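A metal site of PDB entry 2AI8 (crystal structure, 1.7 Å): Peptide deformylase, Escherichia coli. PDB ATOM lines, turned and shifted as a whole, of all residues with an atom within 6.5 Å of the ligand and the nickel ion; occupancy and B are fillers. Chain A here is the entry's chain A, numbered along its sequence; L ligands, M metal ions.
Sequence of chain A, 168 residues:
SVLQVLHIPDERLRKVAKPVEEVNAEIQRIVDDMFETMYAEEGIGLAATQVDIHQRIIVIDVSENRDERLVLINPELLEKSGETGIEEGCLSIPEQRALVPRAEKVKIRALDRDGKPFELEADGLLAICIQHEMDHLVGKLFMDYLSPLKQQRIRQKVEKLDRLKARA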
ATOM      1  N   VAL A   5      19.103 -18.537 -10.233  1.00  0.00           N
ATOM      2  CA  VAL A   5      17.934 -17.818 -10.705  1.00  0.00           C
ATOM      3  C   VAL A   5      17.990 -17.728 -12.220  1.00  0.00           C
ATOM      4  O   VAL A   5      18.983 -17.288 -12.799  1.00  0.00           O
ATOM      5  CB  VAL A   5      17.876 -16.399 -10.111  1.00  0.00           C
ATOM      6  CG1 VAL A   5      16.640 -15.674 -10.604  1.00  0.00           C
ATOM      7  CG2 VAL A   5      17.870 -16.473  -8.592  1.00  0.00           C
ATOM      8  N   MET A  38      16.989 -15.282  -2.351  1.00  0.00           N
ATOM      9  CA  MET A  38      16.558 -13.892  -2.451  1.00  0.00           C
ATOM     10  C   MET A  38      17.503 -12.956  -1.692  1.00  0.00           C
ATOM     11  O   MET A  38      17.925 -11.929  -2.224  1.00  0.00           O
ATOM     12  CB  MET A  38      15.144 -13.742  -1.888  1.00  0.00           C
ATOM     13  CG  MET A  38      14.582 -12.337  -2.022  1.00  0.00           C
ATOM     14  SD  MET A  38      13.084 -12.115  -1.064  1.00  0.00           S
ATOM     15  CE  MET A  38      13.764 -11.862   0.590  1.00  0.00           C
ATOM     16  N   GLU A  42      20.238 -10.186  -3.015  1.00  0.00           N
ATOM     17  CA  GLU A  42      19.773  -8.854  -2.626  1.00  0.00           C
ATOM     18  C   GLU A  42      18.448  -8.416  -3.265  1.00  0.00           C
ATOM     19  O   GLU A  42      18.306  -7.274  -3.699  1.00  0.00           O
ATOM     20  CB  GLU A  42      20.863  -7.815  -2.909  1.00  0.00           C
ATOM     21  CG  GLU A  42      22.222  -8.193  -2.337  1.00  0.00           C
ATOM     22  CD  GLU A  42      23.247  -7.058  -2.416  1.00  0.00           C
ATOM     23  OE1 GLU A  42      23.430  -6.490  -3.509  1.00  0.00           O
ATOM     24  OE2 GLU A  42      23.855  -6.748  -1.377  1.00  0.00           O
ATOM     25  N   GLY A  43      17.487  -9.331  -3.317  1.00  0.00           N
ATOM     26  CA  GLY A  43      16.195  -8.991  -3.883  1.00  0.00           C
ATOM     27  C   GLY A  43      15.184  -8.797  -2.775  1.00  0.00           C
ATOM     28  O   GLY A  43      15.462  -9.115  -1.612  1.00  0.00           O
ATOM     29  N   ILE A  44      14.004  -8.273  -3.116  1.00  0.00           N
ATOM     30  CA  ILE A  44      12.948  -8.068  -2.125  1.00  0.00           C
ATOM     31  C   ILE A  44      11.803  -9.042  -2.375  1.00  0.00           C
ATOM     32  O   ILE A  44      10.815  -9.074  -1.641  1.00  0.00           O
ATOM     33  CB  ILE A  44      12.392  -6.628  -2.153  1.00  0.00           C
ATOM     34  CG1 ILE A  44      11.867  -6.287  -3.543  1.00  0.00           C
ATOM     35  CG2 ILE A  44      13.473  -5.648  -1.715  1.00  0.00           C
ATOM     36  CD1 ILE A  44      11.114  -4.966  -3.596  1.00  0.00           C
ATOM     37  N   GLY A  45      11.961  -9.859  -3.414  1.00  0.00           N
ATOM     38  CA  GLY A  45      10.939 -10.839  -3.745  1.00  0.00           C
ATOM     39  C   GLY A  45      11.496 -11.908  -4.664  1.00  0.00           C
ATOM     40  O   GLY A  45      12.477 -11.677  -5.379  1.00  0.00           O
ATOM     41  N   LEU A  46      10.881 -13.087  -4.645  1.00  0.00           N
ATOM     42  CA  LEU A  46      11.304 -14.170  -5.509  1.00  0.00           C
ATOM     43  C   LEU A  46      10.140 -15.125  -5.682  1.00  0.00           C
ATOM     44  O   LEU A  46       9.444 -15.464  -4.709  1.00  0.00           O
ATOM     45  CB  LEU A  46      12.498 -14.921  -4.904  1.00  0.00           C
ATOM     46  CG  LEU A  46      13.123 -15.997  -5.802  1.00  0.00           C
ATOM     47  CD1 LEU A  46      13.807 -15.354  -6.997  1.00  0.00           C
ATOM     48  CD2 LEU A  46      14.135 -16.811  -5.009  1.00  0.00           C
ATOM     49  N   ALA A  47       9.897 -15.536  -6.919  1.00  0.00           N
ATOM     50  CA  ALA A  47       8.823 -16.474  -7.229  1.00  0.00           C
ATOM     51  C   ALA A  47       9.465 -17.813  -7.577  1.00  0.00           C
ATOM     52  O   ALA A  47      10.537 -17.846  -8.169  1.00  0.00           O
ATOM     53  CB  ALA A  47       7.998 -15.958  -8.404  1.00  0.00           C
ATOM     54  N   GLN A  50      11.075 -18.545 -10.937  1.00  0.00           N
ATOM     55  CA  GLN A  50      12.405 -17.999 -11.180  1.00  0.00           C
ATOM     56  C   GLN A  50      13.541 -18.971 -10.857  1.00  0.00           C
ATOM     57  O   GLN A  50      14.655 -18.802 -11.353  1.00  0.00           O
ATOM     58  CB  GLN A  50      12.616 -16.717 -10.381  1.00  0.00           C
ATOM     59  CG  GLN A  50      11.789 -15.558 -10.862  1.00  0.00           C
ATOM     60  CD  GLN A  50      11.981 -14.324 -10.007  1.00  0.00           C
ATOM     61  OE1 GLN A  50      11.292 -14.139  -9.010  1.00  0.00           O
ATOM     62  NE2 GLN A  50      12.951 -13.491 -10.387  1.00  0.00           N
ATOM     63  N   ILE A  86       6.514   2.250 -10.194  1.00  0.00           N
ATOM     64  CA  ILE A  86       7.844   2.598  -9.705  1.00  0.00           C
ATOM     65  C   ILE A  86       8.817   1.854 -10.614  1.00  0.00           C
ATOM     66  O   ILE A  86       8.410   0.969 -11.363  1.00  0.00           O
ATOM     67  CB  ILE A  86       8.084   2.128  -8.241  1.00  0.00           C
ATOM     68  CG1 ILE A  86       8.029   0.607  -8.152  1.00  0.00           C
ATOM     69  CG2 ILE A  86       7.074   2.779  -7.314  1.00  0.00           C
ATOM     70  CD1 ILE A  86       8.360   0.044  -6.780  1.00  0.00           C
ATOM     71  N   GLU A  87      10.089   2.216 -10.563  1.00  0.00           N
ATOM     72  CA  GLU A  87      11.055   1.531 -11.399  1.00  0.00           C
ATOM     73  C   GLU A  87      11.377   0.186 -10.755  1.00  0.00           C
ATOM     74  O   GLU A  87      12.140   0.099  -9.778  1.00  0.00           O
ATOM     75  CB  GLU A  87      12.307   2.388 -11.571  1.00  0.00           C
ATOM     76  CG  GLU A  87      12.070   3.550 -12.540  1.00  0.00           C
ATOM     77  CD  GLU A  87      13.282   4.423 -12.740  1.00  0.00           C
ATOM     78  OE1 GLU A  87      14.413   3.955 -12.476  1.00  0.00           O
ATOM     79  OE2 GLU A  87      13.106   5.582 -13.193  1.00  0.00           O
ATOM     80  N   GLU A  88      10.778  -0.861 -11.312  1.00  0.00           N
ATOM     81  CA  GLU A  88      10.943  -2.217 -10.811  1.00  0.00           C
ATOM     82  C   GLU A  88      12.185  -2.922 -11.332  1.00  0.00           C
ATOM     83  O   GLU A  88      12.636  -2.675 -12.450  1.00  0.00           O
ATOM     84  CB  GLU A  88       9.721  -3.063 -11.185  1.00  0.00           C
ATOM     85  CG  GLU A  88       8.431  -2.681 -10.462  1.00  0.00           C
ATOM     86  CD  GLU A  88       7.263  -3.555 -10.873  1.00  0.00           C
ATOM     87  OE1 GLU A  88       7.498  -4.731 -11.234  1.00  0.00           O
ATOM     88  OE2 GLU A  88       6.111  -3.071 -10.836  1.00  0.00           O
ATOM     89  N   GLY A  89      12.723  -3.802 -10.501  1.00  0.00           N
ATOM     90  CA  GLY A  89      13.882  -4.583 -10.877  1.00  0.00           C
ATOM     91  C   GLY A  89      13.438  -6.032 -10.804  1.00  0.00           C
ATOM     92  O   GLY A  89      12.310  -6.305 -10.395  1.00  0.00           O
ATOM     93  N   CYS A  90      14.300  -6.957 -11.202  1.00  0.00           N
ATOM     94  CA  CYS A  90      13.966  -8.378 -11.174  1.00  0.00           C
ATOM     95  C   CYS A  90      15.247  -9.186 -11.263  1.00  0.00           C
ATOM     96  O   CYS A  90      16.109  -8.900 -12.097  1.00  0.00           O
ATOM     97  CB  CYS A  90      13.062  -8.738 -12.362  1.00  0.00           C
ATOM     98  SG  CYS A  90      12.519 -10.469 -12.406  1.00  0.00           S
ATOM     99  N   LEU A  91      15.388 -10.182 -10.403  1.00  0.00           N
ATOM    100  CA  LEU A  91      16.584 -11.008 -10.404  1.00  0.00           C
ATOM    101  C   LEU A  91      16.725 -11.829 -11.678  1.00  0.00           C
ATOM    102  O   LEU A  91      17.804 -12.351 -11.970  1.00  0.00           O
ATOM    103  CB  LEU A  91      16.602 -11.931  -9.185  1.00  0.00           C
ATOM    104  CG  LEU A  91      16.713 -11.203  -7.836  1.00  0.00           C
ATOM    105  CD1 LEU A  91      16.597 -12.203  -6.700  1.00  0.00           C
ATOM    106  CD2 LEU A  91      18.043 -10.449  -7.773  1.00  0.00           C
ATOM    107  N   SER A  92      15.637 -11.949 -12.449  1.00  0.00           N
ATOM    108  CA  SER A  92      15.683 -12.689 -13.709  1.00  0.00           C
ATOM    109  C   SER A  92      16.040 -11.752 -14.864  1.00  0.00           C
ATOM    110  O   SER A  92      16.256 -12.194 -15.981  1.00  0.00           O
ATOM    111  CB  SER A  92      14.348 -13.369 -13.973  1.00  0.00           C
ATOM    112  OG  SER A  92      14.124 -14.417 -13.046  1.00  0.00           O
ATOM    113  N   ILE A  93      16.079 -10.450 -14.569  1.00  0.00           N
ATOM    114  CA  ILE A  93      16.443  -9.439 -15.555  1.00  0.00           C
ATOM    115  C   ILE A  93      17.472  -8.587 -14.826  1.00  0.00           C
ATOM    116  O   ILE A  93      17.270  -7.389 -14.594  1.00  0.00           O
ATOM    117  CB  ILE A  93      15.213  -8.575 -15.942  1.00  0.00           C
ATOM    118  CG1 ILE A  93      14.027  -9.476 -16.301  1.00  0.00           C
ATOM    119  CG2 ILE A  93      15.561  -7.678 -17.117  1.00  0.00           C
ATOM    120  CD1 ILE A  93      12.763  -8.727 -16.690  1.00  0.00           C
ATOM    121  N   ARG A  97      16.141  -1.887 -14.699  1.00  0.00           N
ATOM    122  CA  ARG A  97      14.967  -1.392 -13.984  1.00  0.00           C
ATOM    123  C   ARG A  97      14.090  -0.537 -14.898  1.00  0.00           C
ATOM    124  O   ARG A  97      14.594   0.219 -15.722  1.00  0.00           O
ATOM    125  CB  ARG A  97      15.389  -0.580 -12.760  1.00  0.00           C
ATOM    126  CG  ARG A  97      15.819  -1.450 -11.588  1.00  0.00           C
ATOM    127  CD  ARG A  97      16.275  -0.627 -10.386  1.00  0.00           C
ATOM    128  NE  ARG A  97      16.362  -1.461  -9.191  1.00  0.00           N
ATOM    129  CZ  ARG A  97      15.347  -1.693  -8.352  1.00  0.00           C
ATOM    130  NH1 ARG A  97      14.165  -1.136  -8.571  1.00  0.00           N
ATOM    131  NH2 ARG A  97      15.518  -2.488  -7.306  1.00  0.00           N
ATOM    132  N   LEU A 125       4.992  -0.193  -1.730  1.00  0.00           N
ATOM    133  CA  LEU A 125       5.918  -1.146  -2.311  1.00  0.00           C
ATOM    134  C   LEU A 125       5.458  -2.591  -2.194  1.00  0.00           C
ATOM    135  O   LEU A 125       5.612  -3.362  -3.135  1.00  0.00           O
ATOM    136  CB  LEU A 125       7.301  -1.006  -1.665  1.00  0.00           C
ATOM    137  CG  LEU A 125       8.383  -1.965  -2.169  1.00  0.00           C
ATOM    138  CD1 LEU A 125       8.623  -1.739  -3.654  1.00  0.00           C
ATOM    139  CD2 LEU A 125       9.662  -1.730  -1.380  1.00  0.00           C
ATOM    140  N   ILE A 128       2.983  -3.526  -4.904  1.00  0.00           N
ATOM    141  CA  ILE A 128       3.665  -3.647  -6.180  1.00  0.00           C
ATOM    142  C   ILE A 128       4.442  -4.956  -6.259  1.00  0.00           C
ATOM    143  O   ILE A 128       4.380  -5.667  -7.265  1.00  0.00           O
ATOM    144  CB  ILE A 128       4.630  -2.447  -6.402  1.00  0.00           C
ATOM    145  CG1 ILE A 128       3.808  -1.175  -6.628  1.00  0.00           C
ATOM    146  CG2 ILE A 128       5.558  -2.722  -7.586  1.00  0.00           C
ATOM    147  CD1 ILE A 128       4.621   0.109  -6.571  1.00  0.00           C
ATOM    148  N   CYS A 129       5.177  -5.267  -5.206  1.00  0.00           N
ATOM    149  CA  CYS A 129       5.965  -6.494  -5.146  1.00  0.00           C
ATOM    150  C   CYS A 129       5.072  -7.718  -5.299  1.00  0.00           C
ATOM    151  O   CYS A 129       5.387  -8.647  -6.052  1.00  0.00           O
ATOM    152  CB  CYS A 129       6.732  -6.556  -3.825  1.00  0.00           C
ATOM    153  SG  CYS A 129       7.853  -7.962  -3.670  1.00  0.00           S
ATOM    154  N   HIS A 132       4.085  -8.072  -8.887  1.00  0.00           N
ATOM    155  CA  HIS A 132       5.250  -8.467  -9.677  1.00  0.00           C
ATOM    156  C   HIS A 132       5.483  -9.973  -9.522  1.00  0.00           C
ATOM    157  O   HIS A 132       5.636 -10.693 -10.508  1.00  0.00           O
ATOM    158  CB  HIS A 132       6.485  -7.687  -9.178  1.00  0.00           C
ATOM    159  CG  HIS A 132       7.770  -8.091  -9.824  1.00  0.00           C
ATOM    160  ND1 HIS A 132       8.536  -7.224 -10.576  1.00  0.00           N
ATOM    161  CD2 HIS A 132       8.473  -9.258  -9.787  1.00  0.00           C
ATOM    162  CE1 HIS A 132       9.632  -7.825 -10.978  1.00  0.00           C
ATOM    163  NE2 HIS A 132       9.627  -9.067 -10.509  1.00  0.00           N
ATOM    164  N   GLU A 133       5.492 -10.436  -8.280  1.00  0.00           N
ATOM    165  CA  GLU A 133       5.718 -11.852  -8.011  1.00  0.00           C
ATOM    166  C   GLU A 133       4.600 -12.735  -8.553  1.00  0.00           C
ATOM    167  O   GLU A 133       4.870 -13.815  -9.084  1.00  0.00           O
ATOM    168  CB  GLU A 133       5.890 -12.091  -6.512  1.00  0.00           C
ATOM    169  CG  GLU A 133       7.090 -11.379  -5.885  1.00  0.00           C
ATOM    170  CD  GLU A 133       8.352 -11.490  -6.709  1.00  0.00           C
ATOM    171  OE1 GLU A 133       8.561 -12.519  -7.391  1.00  0.00           O
ATOM    172  OE2 GLU A 133       9.161 -10.536  -6.684  1.00  0.00           O
ATOM    173  N   HIS A 136       5.018 -13.512 -12.173  1.00  0.00           N
ATOM    174  CA  HIS A 136       5.970 -14.583 -12.473  1.00  0.00           C
ATOM    175  C   HIS A 136       5.291 -15.941 -12.520  1.00  0.00           C
ATOM    176  O   HIS A 136       5.621 -16.785 -13.358  1.00  0.00           O
ATOM    177  CB  HIS A 136       7.077 -14.643 -11.405  1.00  0.00           C
ATOM    178  CG  HIS A 136       8.199 -13.674 -11.632  1.00  0.00           C
ATOM    179  ND1 HIS A 136       8.964 -13.674 -12.771  1.00  0.00           N
ATOM    180  CD2 HIS A 136       8.704 -12.711 -10.827  1.00  0.00           C
ATOM    181  CE1 HIS A 136       9.896 -12.737 -12.672  1.00  0.00           C
ATOM    182  NE2 HIS A 136       9.759 -12.141 -11.504  1.00  0.00           N
ATOM    183  N   LEU A 141       6.700 -11.162 -17.113  1.00  0.00           N
ATOM    184  CA  LEU A 141       7.848 -10.412 -16.630  1.00  0.00           C
ATOM    185  C   LEU A 141       7.562  -8.916 -16.776  1.00  0.00           C
ATOM    186  O   LEU A 141       6.755  -8.527 -17.618  1.00  0.00           O
ATOM    187  CB  LEU A 141       9.092 -10.782 -17.446  1.00  0.00           C
ATOM    188  CG  LEU A 141       9.431 -12.272 -17.472  1.00  0.00           C
ATOM    189  CD1 LEU A 141      10.507 -12.547 -18.518  1.00  0.00           C
ATOM    190  CD2 LEU A 141       9.896 -12.708 -16.086  1.00  0.00           C
ATOM    191  N   PHE A 142       8.224  -8.073 -15.988  1.00  0.00           N
ATOM    192  CA  PHE A 142       7.945  -6.647 -16.077  1.00  0.00           C
ATOM    193  C   PHE A 142       8.287  -6.041 -17.433  1.00  0.00           C
ATOM    194  O   PHE A 142       7.645  -5.080 -17.871  1.00  0.00           O
ATOM    195  CB  PHE A 142       8.639  -5.866 -14.931  1.00  0.00           C
ATOM    196  CG  PHE A 142      10.101  -5.574 -15.148  1.00  0.00           C
ATOM    197  CD1 PHE A 142      10.517  -4.611 -16.060  1.00  0.00           C
ATOM    198  CD2 PHE A 142      11.066  -6.225 -14.375  1.00  0.00           C
ATOM    199  CE1 PHE A 142      11.858  -4.283 -16.204  1.00  0.00           C
ATOM    200  CE2 PHE A 142      12.416  -5.909 -14.510  1.00  0.00           C
ATOM    201  CZ  PHE A 142      12.820  -4.942 -15.428  1.00  0.00           C
HETATM  202  C1  LIG L   1      11.556  -3.709  -7.291  1.00  0.00           C
HETATM  203  C2  LIG L   1      11.983  -5.064  -7.221  1.00  0.00           C
HETATM  204  C3  LIG L   1      11.028  -6.163  -7.260  1.00  0.00           C
HETATM  205  C4  LIG L   1       9.634  -5.890  -7.367  1.00  0.00           C
HETATM  206  C5  LIG L   1       9.163  -4.572  -7.428  1.00  0.00           C
HETATM  207  C6  LIG L   1      10.187  -3.405  -7.384  1.00  0.00           C
HETATM  208  C7  LIG L   1      11.460  -7.627  -7.168  1.00  0.00           C
HETATM  209  C8  LIG L   1      12.986  -7.830  -7.174  1.00  0.00           C
HETATM  210  C9  LIG L   1      13.503  -9.317  -7.056  1.00  0.00           C
HETATM  211  N1  LIG L   1      12.906 -10.396  -7.994  1.00  0.00           N
HETATM  212  O1  LIG L   1      13.761 -11.228  -8.736  1.00  0.00           O
HETATM  213  C10 LIG L   1      11.552 -10.579  -8.085  1.00  0.00           C
HETATM  214  O2  LIG L   1      10.903 -11.567  -8.896  1.00  0.00           O
HETATM  215 NI    NI M   1      10.896 -10.665 -10.748  1.00  0.00          NI
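Residues that only touch the nickel ion: Gln 50.
Of the 26 residues printed, 4 come within 4 Å of the nickel ion.
The nearest printed residue that does not touch the nickel ion is Glu 133 (4.4 Å).
The nickel ion is bound by NE2 of His 136 (2.0 Å).
The nickel ion is bound by NE2 of His 132 (2.1 Å).
The nickel ion is bound by O2 of the ligand, 2.1 Å away.
The side-chain sulfur (SG) of Cys 90 is bound to the nickel ion, 2.3 Å away.
The nickel ion has four donor atoms within binding distance.
SG of Cys 90 lies close to NE2 of Gln 50 (3.7 Å).
N of Ser 92 lies close to SG of Cys 90 (3.5 Å).
NE2 of Gln 50 is in hydrogen-bond range of OG of Ser 92 (3.1 Å).
The backbone NH (N) of Ala 47 lies within hydrogen-bond range of the side-chain amide oxygen (OE1) of Gln 50 (2.9 Å).
N of Ala 47 lies within hydrogen-bond range of OE1 of Glu 133 (3.3 Å).
SD of Met 38 sits at hydrogen-bond distance from N of Gly 45 (3.4 Å).
The backbone carbonyl oxygen of Ile 44 is in hydrogen-bond range of the side-chain sulfur of Cys 129 (3.8 Å).
The guanidinium group of Arg 97 lies within hydrogen-bond range of the backbone carbonyl oxygen of Glu 87.
The backbone NH of Leu 91 sits at hydrogen-bond distance from an oxygen (O1) of the ligand (2.6 Å).
NE2 of Gln 50 is in hydrogen-bond range of O1 of the ligand.
An oxygen (O2) of the ligand lies close to the side-chain carboxylate (OE1) of Glu 133, at 2.9 Å.
The backbone carbonyl oxygen (O) of Gly 45 sits close to a nitrogen (N1) of the ligand (2.9 Å).
Residues that only touch the ligand: Gly 89, Glu 88, Ile 44, Arg 97 and Ile 86.
Hydrophobic or aromatic side chains that line the ligand: Ile 44, Ile 86, Leu 91, His 132 and His 136.
Of the 26 residues printed, 12 come within 4 Å of the ligand.
The nearest printed residue that does not touch the ligand is Ile 128 (4.1 Å).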
